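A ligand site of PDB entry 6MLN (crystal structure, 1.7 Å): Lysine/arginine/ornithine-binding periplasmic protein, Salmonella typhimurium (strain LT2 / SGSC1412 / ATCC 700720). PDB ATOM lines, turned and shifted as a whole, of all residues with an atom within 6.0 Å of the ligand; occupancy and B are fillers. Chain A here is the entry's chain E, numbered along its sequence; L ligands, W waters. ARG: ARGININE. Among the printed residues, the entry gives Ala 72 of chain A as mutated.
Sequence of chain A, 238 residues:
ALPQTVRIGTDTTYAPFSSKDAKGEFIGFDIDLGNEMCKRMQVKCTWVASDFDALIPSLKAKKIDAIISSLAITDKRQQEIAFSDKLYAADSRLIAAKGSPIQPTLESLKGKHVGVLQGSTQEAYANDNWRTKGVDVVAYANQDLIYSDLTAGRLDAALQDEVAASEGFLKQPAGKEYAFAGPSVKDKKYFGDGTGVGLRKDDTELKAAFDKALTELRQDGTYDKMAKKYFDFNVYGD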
ATOM      1  N   THR A  10      17.055 -16.489  26.640  1.00  0.00           N
ATOM      2  CA  THR A  10      16.933 -17.797  25.997  1.00  0.00           C
ATOM      3  C   THR A  10      15.817 -17.760  24.952  1.00  0.00           C
ATOM      4  O   THR A  10      14.889 -16.968  25.062  1.00  0.00           O
ATOM      5  CB  THR A  10      16.652 -18.898  27.051  1.00  0.00           C
ATOM      6  OG1 THR A  10      16.785 -20.206  26.461  1.00  0.00           O
ATOM      7  CG2 THR A  10      15.242 -18.740  27.666  1.00  0.00           C
ATOM      8  N   ASP A  11      15.932 -18.607  23.933  1.00  0.00           N
ATOM      9  CA  ASP A  11      14.814 -18.822  23.018  1.00  0.00           C
ATOM     10  C   ASP A  11      14.103 -20.094  23.395  1.00  0.00           C
ATOM     11  O   ASP A  11      14.712 -21.169  23.459  1.00  0.00           O
ATOM     12  CB  ASP A  11      15.262 -18.891  21.566  1.00  0.00           C
ATOM     13  CG  ASP A  11      14.215 -19.531  20.680  1.00  0.00           C
ATOM     14  OD1 ASP A  11      13.236 -18.834  20.316  1.00  0.00           O
ATOM     15  OD2 ASP A  11      14.326 -20.739  20.392  1.00  0.00           O
ATOM     16  N   THR A  12      12.794 -19.996  23.601  1.00  0.00           N
ATOM     17  CA  THR A  12      12.027 -21.103  24.157  1.00  0.00           C
ATOM     18  C   THR A  12      11.324 -21.941  23.089  1.00  0.00           C
ATOM     19  O   THR A  12      10.226 -22.454  23.310  1.00  0.00           O
ATOM     20  CB  THR A  12      10.992 -20.581  25.170  1.00  0.00           C
ATOM     21  OG1 THR A  12      10.141 -19.623  24.530  1.00  0.00           O
ATOM     22  CG2 THR A  12      11.711 -19.892  26.348  1.00  0.00           C
ATOM     23  N   THR A  13      11.955 -22.134  21.939  1.00  0.00           N
ATOM     24  CA  THR A  13      11.368 -23.020  20.930  1.00  0.00           C
ATOM     25  C   THR A  13      12.288 -24.207  20.633  1.00  0.00           C
ATOM     26  O   THR A  13      12.275 -24.744  19.531  1.00  0.00           O
ATOM     27  CB  THR A  13      11.037 -22.269  19.611  1.00  0.00           C
ATOM     28  OG1 THR A  13      12.230 -21.780  18.990  1.00  0.00           O
ATOM     29  CG2 THR A  13      10.112 -21.099  19.895  1.00  0.00           C
ATOM     30  N   TYR A  14      13.045 -24.633  21.636  1.00  0.00           N
ATOM     31  CA  TYR A  14      14.075 -25.643  21.390  1.00  0.00           C
ATOM     32  C   TYR A  14      14.062 -26.740  22.477  1.00  0.00           C
ATOM     33  O   TYR A  14      15.059 -26.985  23.162  1.00  0.00           O
ATOM     34  CB  TYR A  14      15.441 -24.943  21.328  1.00  0.00           C
ATOM     35  CG  TYR A  14      16.315 -25.344  20.157  1.00  0.00           C
ATOM     36  CD1 TYR A  14      15.894 -25.136  18.844  1.00  0.00           C
ATOM     37  CD2 TYR A  14      17.595 -25.860  20.367  1.00  0.00           C
ATOM     38  CE1 TYR A  14      16.716 -25.475  17.758  1.00  0.00           C
ATOM     39  CE2 TYR A  14      18.421 -26.205  19.294  1.00  0.00           C
ATOM     40  CZ  TYR A  14      17.977 -26.001  18.004  1.00  0.00           C
ATOM     41  OH  TYR A  14      18.818 -26.339  16.968  1.00  0.00           O
ATOM     42  N   SER A  18      15.201 -25.711  25.918  1.00  0.00           N
ATOM     43  CA  SER A  18      14.503 -24.495  26.349  1.00  0.00           C
ATOM     44  C   SER A  18      13.150 -24.435  25.666  1.00  0.00           C
ATOM     45  O   SER A  18      13.072 -24.319  24.450  1.00  0.00           O
ATOM     46  CB  SER A  18      15.338 -23.252  26.020  1.00  0.00           C
ATOM     47  OG  SER A  18      14.708 -22.065  26.519  1.00  0.00           O
ATOM     48  N   ASP A  30      18.544 -26.528  29.581  1.00  0.00           N
ATOM     49  CA  ASP A  30      19.175 -25.200  29.701  1.00  0.00           C
ATOM     50  C   ASP A  30      18.680 -24.462  30.941  1.00  0.00           C
ATOM     51  O   ASP A  30      19.461 -23.824  31.663  1.00  0.00           O
ATOM     52  CB  ASP A  30      18.897 -24.313  28.484  1.00  0.00           C
ATOM     53  CG  ASP A  30      19.816 -24.590  27.309  1.00  0.00           C
ATOM     54  OD1 ASP A  30      20.798 -25.323  27.455  1.00  0.00           O
ATOM     55  OD2 ASP A  30      19.545 -24.040  26.223  1.00  0.00           O
ATOM     56  N   PHE A  52      15.960 -16.346  18.907  1.00  0.00           N
ATOM     57  CA  PHE A  52      17.359 -16.745  18.970  1.00  0.00           C
ATOM     58  C   PHE A  52      18.289 -15.703  18.369  1.00  0.00           C
ATOM     59  O   PHE A  52      19.345 -15.399  18.939  1.00  0.00           O
ATOM     60  CB  PHE A  52      17.563 -18.085  18.285  1.00  0.00           C
ATOM     61  CG  PHE A  52      18.956 -18.626  18.428  1.00  0.00           C
ATOM     62  CD1 PHE A  52      19.362 -19.214  19.619  1.00  0.00           C
ATOM     63  CD2 PHE A  52      19.873 -18.510  17.386  1.00  0.00           C
ATOM     64  CE1 PHE A  52      20.645 -19.697  19.777  1.00  0.00           C
ATOM     65  CE2 PHE A  52      21.162 -18.998  17.532  1.00  0.00           C
ATOM     66  CZ  PHE A  52      21.552 -19.581  18.739  1.00  0.00           C
ATOM     67  N   LEU A  55      19.516 -12.765  20.630  1.00  0.00           N
ATOM     68  CA  LEU A  55      20.205 -13.015  21.893  1.00  0.00           C
ATOM     69  C   LEU A  55      21.561 -12.311  21.974  1.00  0.00           C
ATOM     70  O   LEU A  55      21.823 -11.587  22.927  1.00  0.00           O
ATOM     71  CB  LEU A  55      20.371 -14.524  22.121  1.00  0.00           C
ATOM     72  CG  LEU A  55      19.051 -15.216  22.477  1.00  0.00           C
ATOM     73  CD1 LEU A  55      19.168 -16.730  22.316  1.00  0.00           C
ATOM     74  CD2 LEU A  55      18.599 -14.868  23.894  1.00  0.00           C
ATOM     75  N   SER A  69      21.048 -20.992  25.788  1.00  0.00           N
ATOM     76  CA  SER A  69      20.077 -21.208  24.723  1.00  0.00           C
ATOM     77  C   SER A  69      20.649 -22.141  23.648  1.00  0.00           C
ATOM     78  O   SER A  69      20.518 -21.861  22.446  1.00  0.00           O
ATOM     79  CB  SER A  69      19.701 -19.848  24.120  1.00  0.00           C
ATOM     80  OG  SER A  69      18.504 -19.945  23.356  1.00  0.00           O
ATOM     81  N   SER A  70      21.263 -23.241  24.096  1.00  0.00           N
ATOM     82  CA  SER A  70      22.016 -24.145  23.217  1.00  0.00           C
ATOM     83  C   SER A  70      22.978 -23.352  22.323  1.00  0.00           C
ATOM     84  O   SER A  70      23.141 -23.664  21.130  1.00  0.00           O
ATOM     85  CB  SER A  70      21.080 -25.012  22.359  1.00  0.00           C
ATOM     86  OG  SER A  70      20.238 -25.856  23.149  1.00  0.00           O
ATOM     87  N   LEU A  71      23.591 -22.314  22.876  1.00  0.00           N
ATOM     88  CA  LEU A  71      24.418 -21.402  22.096  1.00  0.00           C
ATOM     89  C   LEU A  71      25.801 -21.999  21.847  1.00  0.00           C
ATOM     90  O   LEU A  71      26.618 -22.088  22.752  1.00  0.00           O
ATOM     91  CB  LEU A  71      24.541 -20.048  22.798  1.00  0.00           C
ATOM     92  CG  LEU A  71      25.276 -18.952  22.015  1.00  0.00           C
ATOM     93  CD1 LEU A  71      24.412 -18.483  20.835  1.00  0.00           C
ATOM     94  CD2 LEU A  71      25.627 -17.792  22.941  1.00  0.00           C
ATOM     95  N   ALA A  72      26.030 -22.452  20.612  1.00  0.00           N
ATOM     96  CA  ALA A  72      27.280 -23.115  20.270  1.00  0.00           C
ATOM     97  C   ALA A  72      28.479 -22.182  20.399  1.00  0.00           C
ATOM     98  O   ALA A  72      28.417 -20.995  20.047  1.00  0.00           O
ATOM     99  CB  ALA A  72      27.201 -23.694  18.851  1.00  0.00           C
ATOM    100  N   ILE A  73      29.562 -22.729  20.911  1.00  0.00           N
ATOM    101  CA  ILE A  73      30.813 -22.010  21.084  1.00  0.00           C
ATOM    102  C   ILE A  73      31.594 -22.065  19.777  1.00  0.00           C
ATOM    103  O   ILE A  73      32.249 -23.060  19.470  1.00  0.00           O
ATOM    104  CB  ILE A  73      31.659 -22.630  22.224  1.00  0.00           C
ATOM    105  CG1 ILE A  73      30.830 -22.746  23.501  1.00  0.00           C
ATOM    106  CG2 ILE A  73      32.910 -21.793  22.471  1.00  0.00           C
ATOM    107  CD1 ILE A  73      31.456 -23.621  24.564  1.00  0.00           C
ATOM    108  N   ARG A  77      31.708 -16.485  16.986  1.00  0.00           N
ATOM    109  CA  ARG A  77      31.034 -15.896  18.132  1.00  0.00           C
ATOM    110  C   ARG A  77      32.018 -15.444  19.211  1.00  0.00           C
ATOM    111  O   ARG A  77      31.776 -14.433  19.877  1.00  0.00           O
ATOM    112  CB  ARG A  77      30.004 -16.870  18.717  1.00  0.00           C
ATOM    113  CG  ARG A  77      28.773 -16.987  17.835  1.00  0.00           C
ATOM    114  CD  ARG A  77      27.888 -18.112  18.305  1.00  0.00           C
ATOM    115  NE  ARG A  77      26.692 -18.188  17.484  1.00  0.00           N
ATOM    116  CZ  ARG A  77      25.847 -19.211  17.481  1.00  0.00           C
ATOM    117  NH1 ARG A  77      26.081 -20.266  18.254  1.00  0.00           N
ATOM    118  NH2 ARG A  77      24.770 -19.174  16.713  1.00  0.00           N
ATOM    119  N   ALA A  90      26.724 -30.545  20.924  1.00  0.00           N
ATOM    120  CA  ALA A  90      25.584 -30.361  20.030  1.00  0.00           C
ATOM    121  C   ALA A  90      25.958 -30.597  18.568  1.00  0.00           C
ATOM    122  O   ALA A  90      26.536 -29.724  17.925  1.00  0.00           O
ATOM    123  CB  ALA A  90      24.985 -28.960  20.196  1.00  0.00           C
ATOM    124  N   LEU A 117      16.951 -22.213  11.462  1.00  0.00           N
ATOM    125  CA  LEU A 117      16.697 -21.133  12.403  1.00  0.00           C
ATOM    126  C   LEU A 117      17.548 -19.892  12.091  1.00  0.00           C
ATOM    127  O   LEU A 117      18.768 -19.980  11.962  1.00  0.00           O
ATOM    128  CB  LEU A 117      16.967 -21.620  13.823  1.00  0.00           C
ATOM    129  CG  LEU A 117      16.884 -20.587  14.941  1.00  0.00           C
ATOM    130  CD1 LEU A 117      15.450 -20.093  15.036  1.00  0.00           C
ATOM    131  CD2 LEU A 117      17.336 -21.257  16.235  1.00  0.00           C
ATOM    132  N   GLY A 119      19.877 -16.916  12.468  1.00  0.00           N
ATOM    133  CA  GLY A 119      20.903 -16.600  13.443  1.00  0.00           C
ATOM    134  C   GLY A 119      21.681 -17.813  13.938  1.00  0.00           C
ATOM    135  O   GLY A 119      22.611 -17.674  14.728  1.00  0.00           O
ATOM    136  N   SER A 120      21.301 -19.000  13.480  1.00  0.00           N
ATOM    137  CA  SER A 120      21.932 -20.227  13.957  1.00  0.00           C
ATOM    138  C   SER A 120      23.159 -20.647  13.160  1.00  0.00           C
ATOM    139  O   SER A 120      23.393 -20.181  12.034  1.00  0.00           O
ATOM    140  CB  SER A 120      20.918 -21.385  13.942  1.00  0.00           C
ATOM    141  OG  SER A 120      20.589 -21.763  12.609  1.00  0.00           O
ATOM    142  N   THR A 121      23.952 -21.532  13.755  1.00  0.00           N
ATOM    143  CA  THR A 121      25.041 -22.186  13.039  1.00  0.00           C
ATOM    144  C   THR A 121      24.496 -22.968  11.848  1.00  0.00           C
ATOM    145  O   THR A 121      25.164 -23.064  10.815  1.00  0.00           O
ATOM    146  CB  THR A 121      25.817 -23.143  13.965  1.00  0.00           C
ATOM    147  OG1 THR A 121      24.914 -24.083  14.543  1.00  0.00           O
ATOM    148  CG2 THR A 121      26.515 -22.352  15.080  1.00  0.00           C
ATOM    149  N   GLN A 122      23.298 -23.522  11.975  1.00  0.00           N
ATOM    150  CA  GLN A 122      22.685 -24.249  10.856  1.00  0.00           C
ATOM    151  C   GLN A 122      22.396 -23.310   9.690  1.00  0.00           C
ATOM    152  O   GLN A 122      22.601 -23.671   8.527  1.00  0.00           O
ATOM    153  CB  GLN A 122      21.399 -24.942  11.304  1.00  0.00           C
ATOM    154  CG  GLN A 122      21.647 -26.138  12.208  1.00  0.00           C
ATOM    155  CD  GLN A 122      21.778 -25.742  13.669  1.00  0.00           C
ATOM    156  OE1 GLN A 122      21.462 -24.622  14.043  1.00  0.00           O
ATOM    157  NE2 GLN A 122      22.243 -26.667  14.503  1.00  0.00           N
ATOM    158  N   GLN A 143      12.205 -22.037  15.892  1.00  0.00           N
ATOM    159  CA  GLN A 143      12.206 -23.445  15.470  1.00  0.00           C
ATOM    160  C   GLN A 143      10.795 -24.062  15.405  1.00  0.00           C
ATOM    161  O   GLN A 143      10.567 -25.025  14.679  1.00  0.00           O
ATOM    162  CB  GLN A 143      13.118 -24.261  16.407  1.00  0.00           C
ATOM    163  CG  GLN A 143      13.281 -25.751  16.054  1.00  0.00           C
ATOM    164  CD  GLN A 143      14.131 -25.990  14.806  1.00  0.00           C
ATOM    165  OE1 GLN A 143      15.081 -25.262  14.542  1.00  0.00           O
ATOM    166  NE2 GLN A 143      13.780 -27.018  14.040  1.00  0.00           N
ATOM    167  N   ASP A 161      19.860 -28.645  15.753  1.00  0.00           N
ATOM    168  CA  ASP A 161      20.623 -29.524  16.636  1.00  0.00           C
ATOM    169  C   ASP A 161      19.958 -30.903  16.717  1.00  0.00           C
ATOM    170  O   ASP A 161      18.733 -31.011  16.823  1.00  0.00           O
ATOM    171  CB  ASP A 161      20.773 -28.930  18.044  1.00  0.00           C
ATOM    172  CG  ASP A 161      21.723 -27.736  18.113  1.00  0.00           C
ATOM    173  OD1 ASP A 161      22.516 -27.501  17.158  1.00  0.00           O
ATOM    174  OD2 ASP A 161      21.705 -27.056  19.149  1.00  0.00           O
ATOM    175  N   PHE A 191      29.712 -25.611  13.422  1.00  0.00           N
ATOM    176  CA  PHE A 191      28.749 -25.927  14.470  1.00  0.00           C
ATOM    177  C   PHE A 191      29.293 -25.772  15.882  1.00  0.00           C
ATOM    178  O   PHE A 191      28.551 -25.907  16.853  1.00  0.00           O
ATOM    179  CB  PHE A 191      28.191 -27.334  14.241  1.00  0.00           C
ATOM    180  CG  PHE A 191      27.499 -27.480  12.918  1.00  0.00           C
ATOM    181  CD1 PHE A 191      26.389 -26.704  12.627  1.00  0.00           C
ATOM    182  CD2 PHE A 191      27.979 -28.364  11.962  1.00  0.00           C
ATOM    183  CE1 PHE A 191      25.752 -26.807  11.390  1.00  0.00           C
ATOM    184  CE2 PHE A 191      27.344 -28.486  10.733  1.00  0.00           C
ATOM    185  CZ  PHE A 191      26.237 -27.706  10.450  1.00  0.00           C
ATOM    186  N   THR A 195      28.031 -26.253  23.483  1.00  0.00           N
ATOM    187  CA  THR A 195      27.332 -25.010  23.821  1.00  0.00           C
ATOM    188  C   THR A 195      27.863 -24.462  25.137  1.00  0.00           C
ATOM    189  O   THR A 195      28.461 -25.198  25.913  1.00  0.00           O
ATOM    190  CB  THR A 195      25.807 -25.208  23.932  1.00  0.00           C
ATOM    191  OG1 THR A 195      25.507 -26.020  25.082  1.00  0.00           O
ATOM    192  CG2 THR A 195      25.271 -25.866  22.670  1.00  0.00           C
HETATM  193  N   ARG L   1      23.249 -24.767  18.373  1.00  0.00           N
HETATM  194  CA  ARG L   1      22.722 -23.875  17.345  1.00  0.00           C
HETATM  195  C   ARG L   1      23.426 -22.532  17.429  1.00  0.00           C
HETATM  196  O   ARG L   1      24.189 -22.288  18.363  1.00  0.00           O
HETATM  197  CB  ARG L   1      21.206 -23.693  17.476  1.00  0.00           C
HETATM  198  CG  ARG L   1      20.777 -23.256  18.889  1.00  0.00           C
HETATM  199  CD  ARG L   1      19.326 -22.763  18.909  1.00  0.00           C
HETATM  200  NE  ARG L   1      18.827 -22.616  20.274  1.00  0.00           N
HETATM  201  CZ  ARG L   1      17.603 -22.209  20.596  1.00  0.00           C
HETATM  202  NH1 ARG L   1      16.727 -21.892  19.655  1.00  0.00           N
HETATM  203  NH2 ARG L   1      17.242 -22.124  21.878  1.00  0.00           N
HETATM  204  OXT ARG L   1      23.253 -21.686  16.553  1.00  0.00           O
HETATM  205  O   HOH W   1      25.677 -25.607  16.626  1.00  0.00           O
HETATM  206  O   HOH W   2      18.167 -24.055  23.772  1.00  0.00           O
HETATM  207  O   HOH W   3      18.888 -24.529  15.035  1.00  0.00           O
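A nitrogen (NH2) of the ligand sits at hydrogen-bond distance from the backbone carbonyl oxygen of Asp 11. The side-chain carboxylate of Asp 11 is in salt-bridge range of a nitrogen (NH1) of the ligand, 2.8 Å away. The guanidinium group (NH1) of Arg 77 lies within salt-bridge range of an oxygen (O) of the ligand, at 2.8 Å. O of Ser 69 sits at hydrogen-bond distance from NE of the ligand, at 2.9 Å. The side-chain hydroxyl (OG) of Ser 69 lies within hydrogen-bond range of a nitrogen (NH2) of the ligand (2.9 Å). The side-chain carboxylate of Asp 161 lies within salt-bridge range of a nitrogen (N) of the ligand (2.9 Å). The backbone NH of Thr 121 lies within hydrogen-bond range of an oxygen (OXT) of the ligand, at 2.9 Å. The backbone NH of Ala 72 is in hydrogen-bond range of an oxygen (O) of the ligand, at 2.9 Å. The backbone carbonyl oxygen (O) of Ser 70 lies within hydrogen-bond range of a nitrogen (N) of the ligand (3.0 Å).
OG of Ser 69 sits at hydrogen-bond distance from N of Asp 11. The guanidinium group of Arg 77 is in hydrogen-bond range of the backbone carbonyl oxygen of Ala 72 (3.0 Å). The guanidinium group (NH2) of Arg 77 sits at hydrogen-bond distance from the backbone carbonyl oxygen (O) of Gly 119 (3.3 Å). N of Ser 69 sits close to OD2 of Asp 30, 3.4 Å away. N of Asp 161 sits at hydrogen-bond distance from OH of Tyr 14, at 2.8 Å. NE2 of Gln 122 lies within hydrogen-bond range of OD1 of Asp 161. OG of Ser 120 is in hydrogen-bond range of O of Leu 117 (2.6 Å). The side-chain hydroxyl of Ser 120 lies close to the backbone NH of Gln 122, 3.3 Å away.
Tyr 14 touches the ligand (CB to NH2, 3.4 Å). Phe 52 touches the ligand (CE1 to CD, 3.4 Å). Leu 71 touches the ligand (CA to O, 3.8 Å). Leu 117 touches the ligand. Ser 120 touches the ligand (CA to OXT, 3.3 Å). OE1 of Gln 122 touches CB of the ligand, at 3.6 Å. Hydrophobic or aromatic side chains within 4 Å of the ligand: Tyr 14, Phe 52, Ala 72 and Leu 117. Within 4 Å of the ligand: Asp 11, Tyr 14, Phe 52, Ser 69, Ser 70, Leu 71, Ala 72, Arg 77, Leu 117, Ser 120, Thr 121, Gln 122 and Asp 161. The nearest printed residue that does not touch the ligand is Gly 119 (4.5 Å).
Water W2 lies within hydrogen-bond range of OD2 of Asp 30 (2.8 Å), OG of Ser 70 (2.8 Å), NH2 of the ligand (2.9 Å) and O of Ser 69 (3.5 Å). Water W1 lies within hydrogen-bond range of the side-chain hydroxyl (OG1) of Thr 121 (2.7 Å), the backbone carbonyl oxygen (O) of Phe 191 (2.9 Å) and a nitrogen (N) of the ligand (3.1 Å). Water W3 bridges OH of Tyr 14 (2.6 Å) and OE1 of Gln 122 (2.8 Å).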
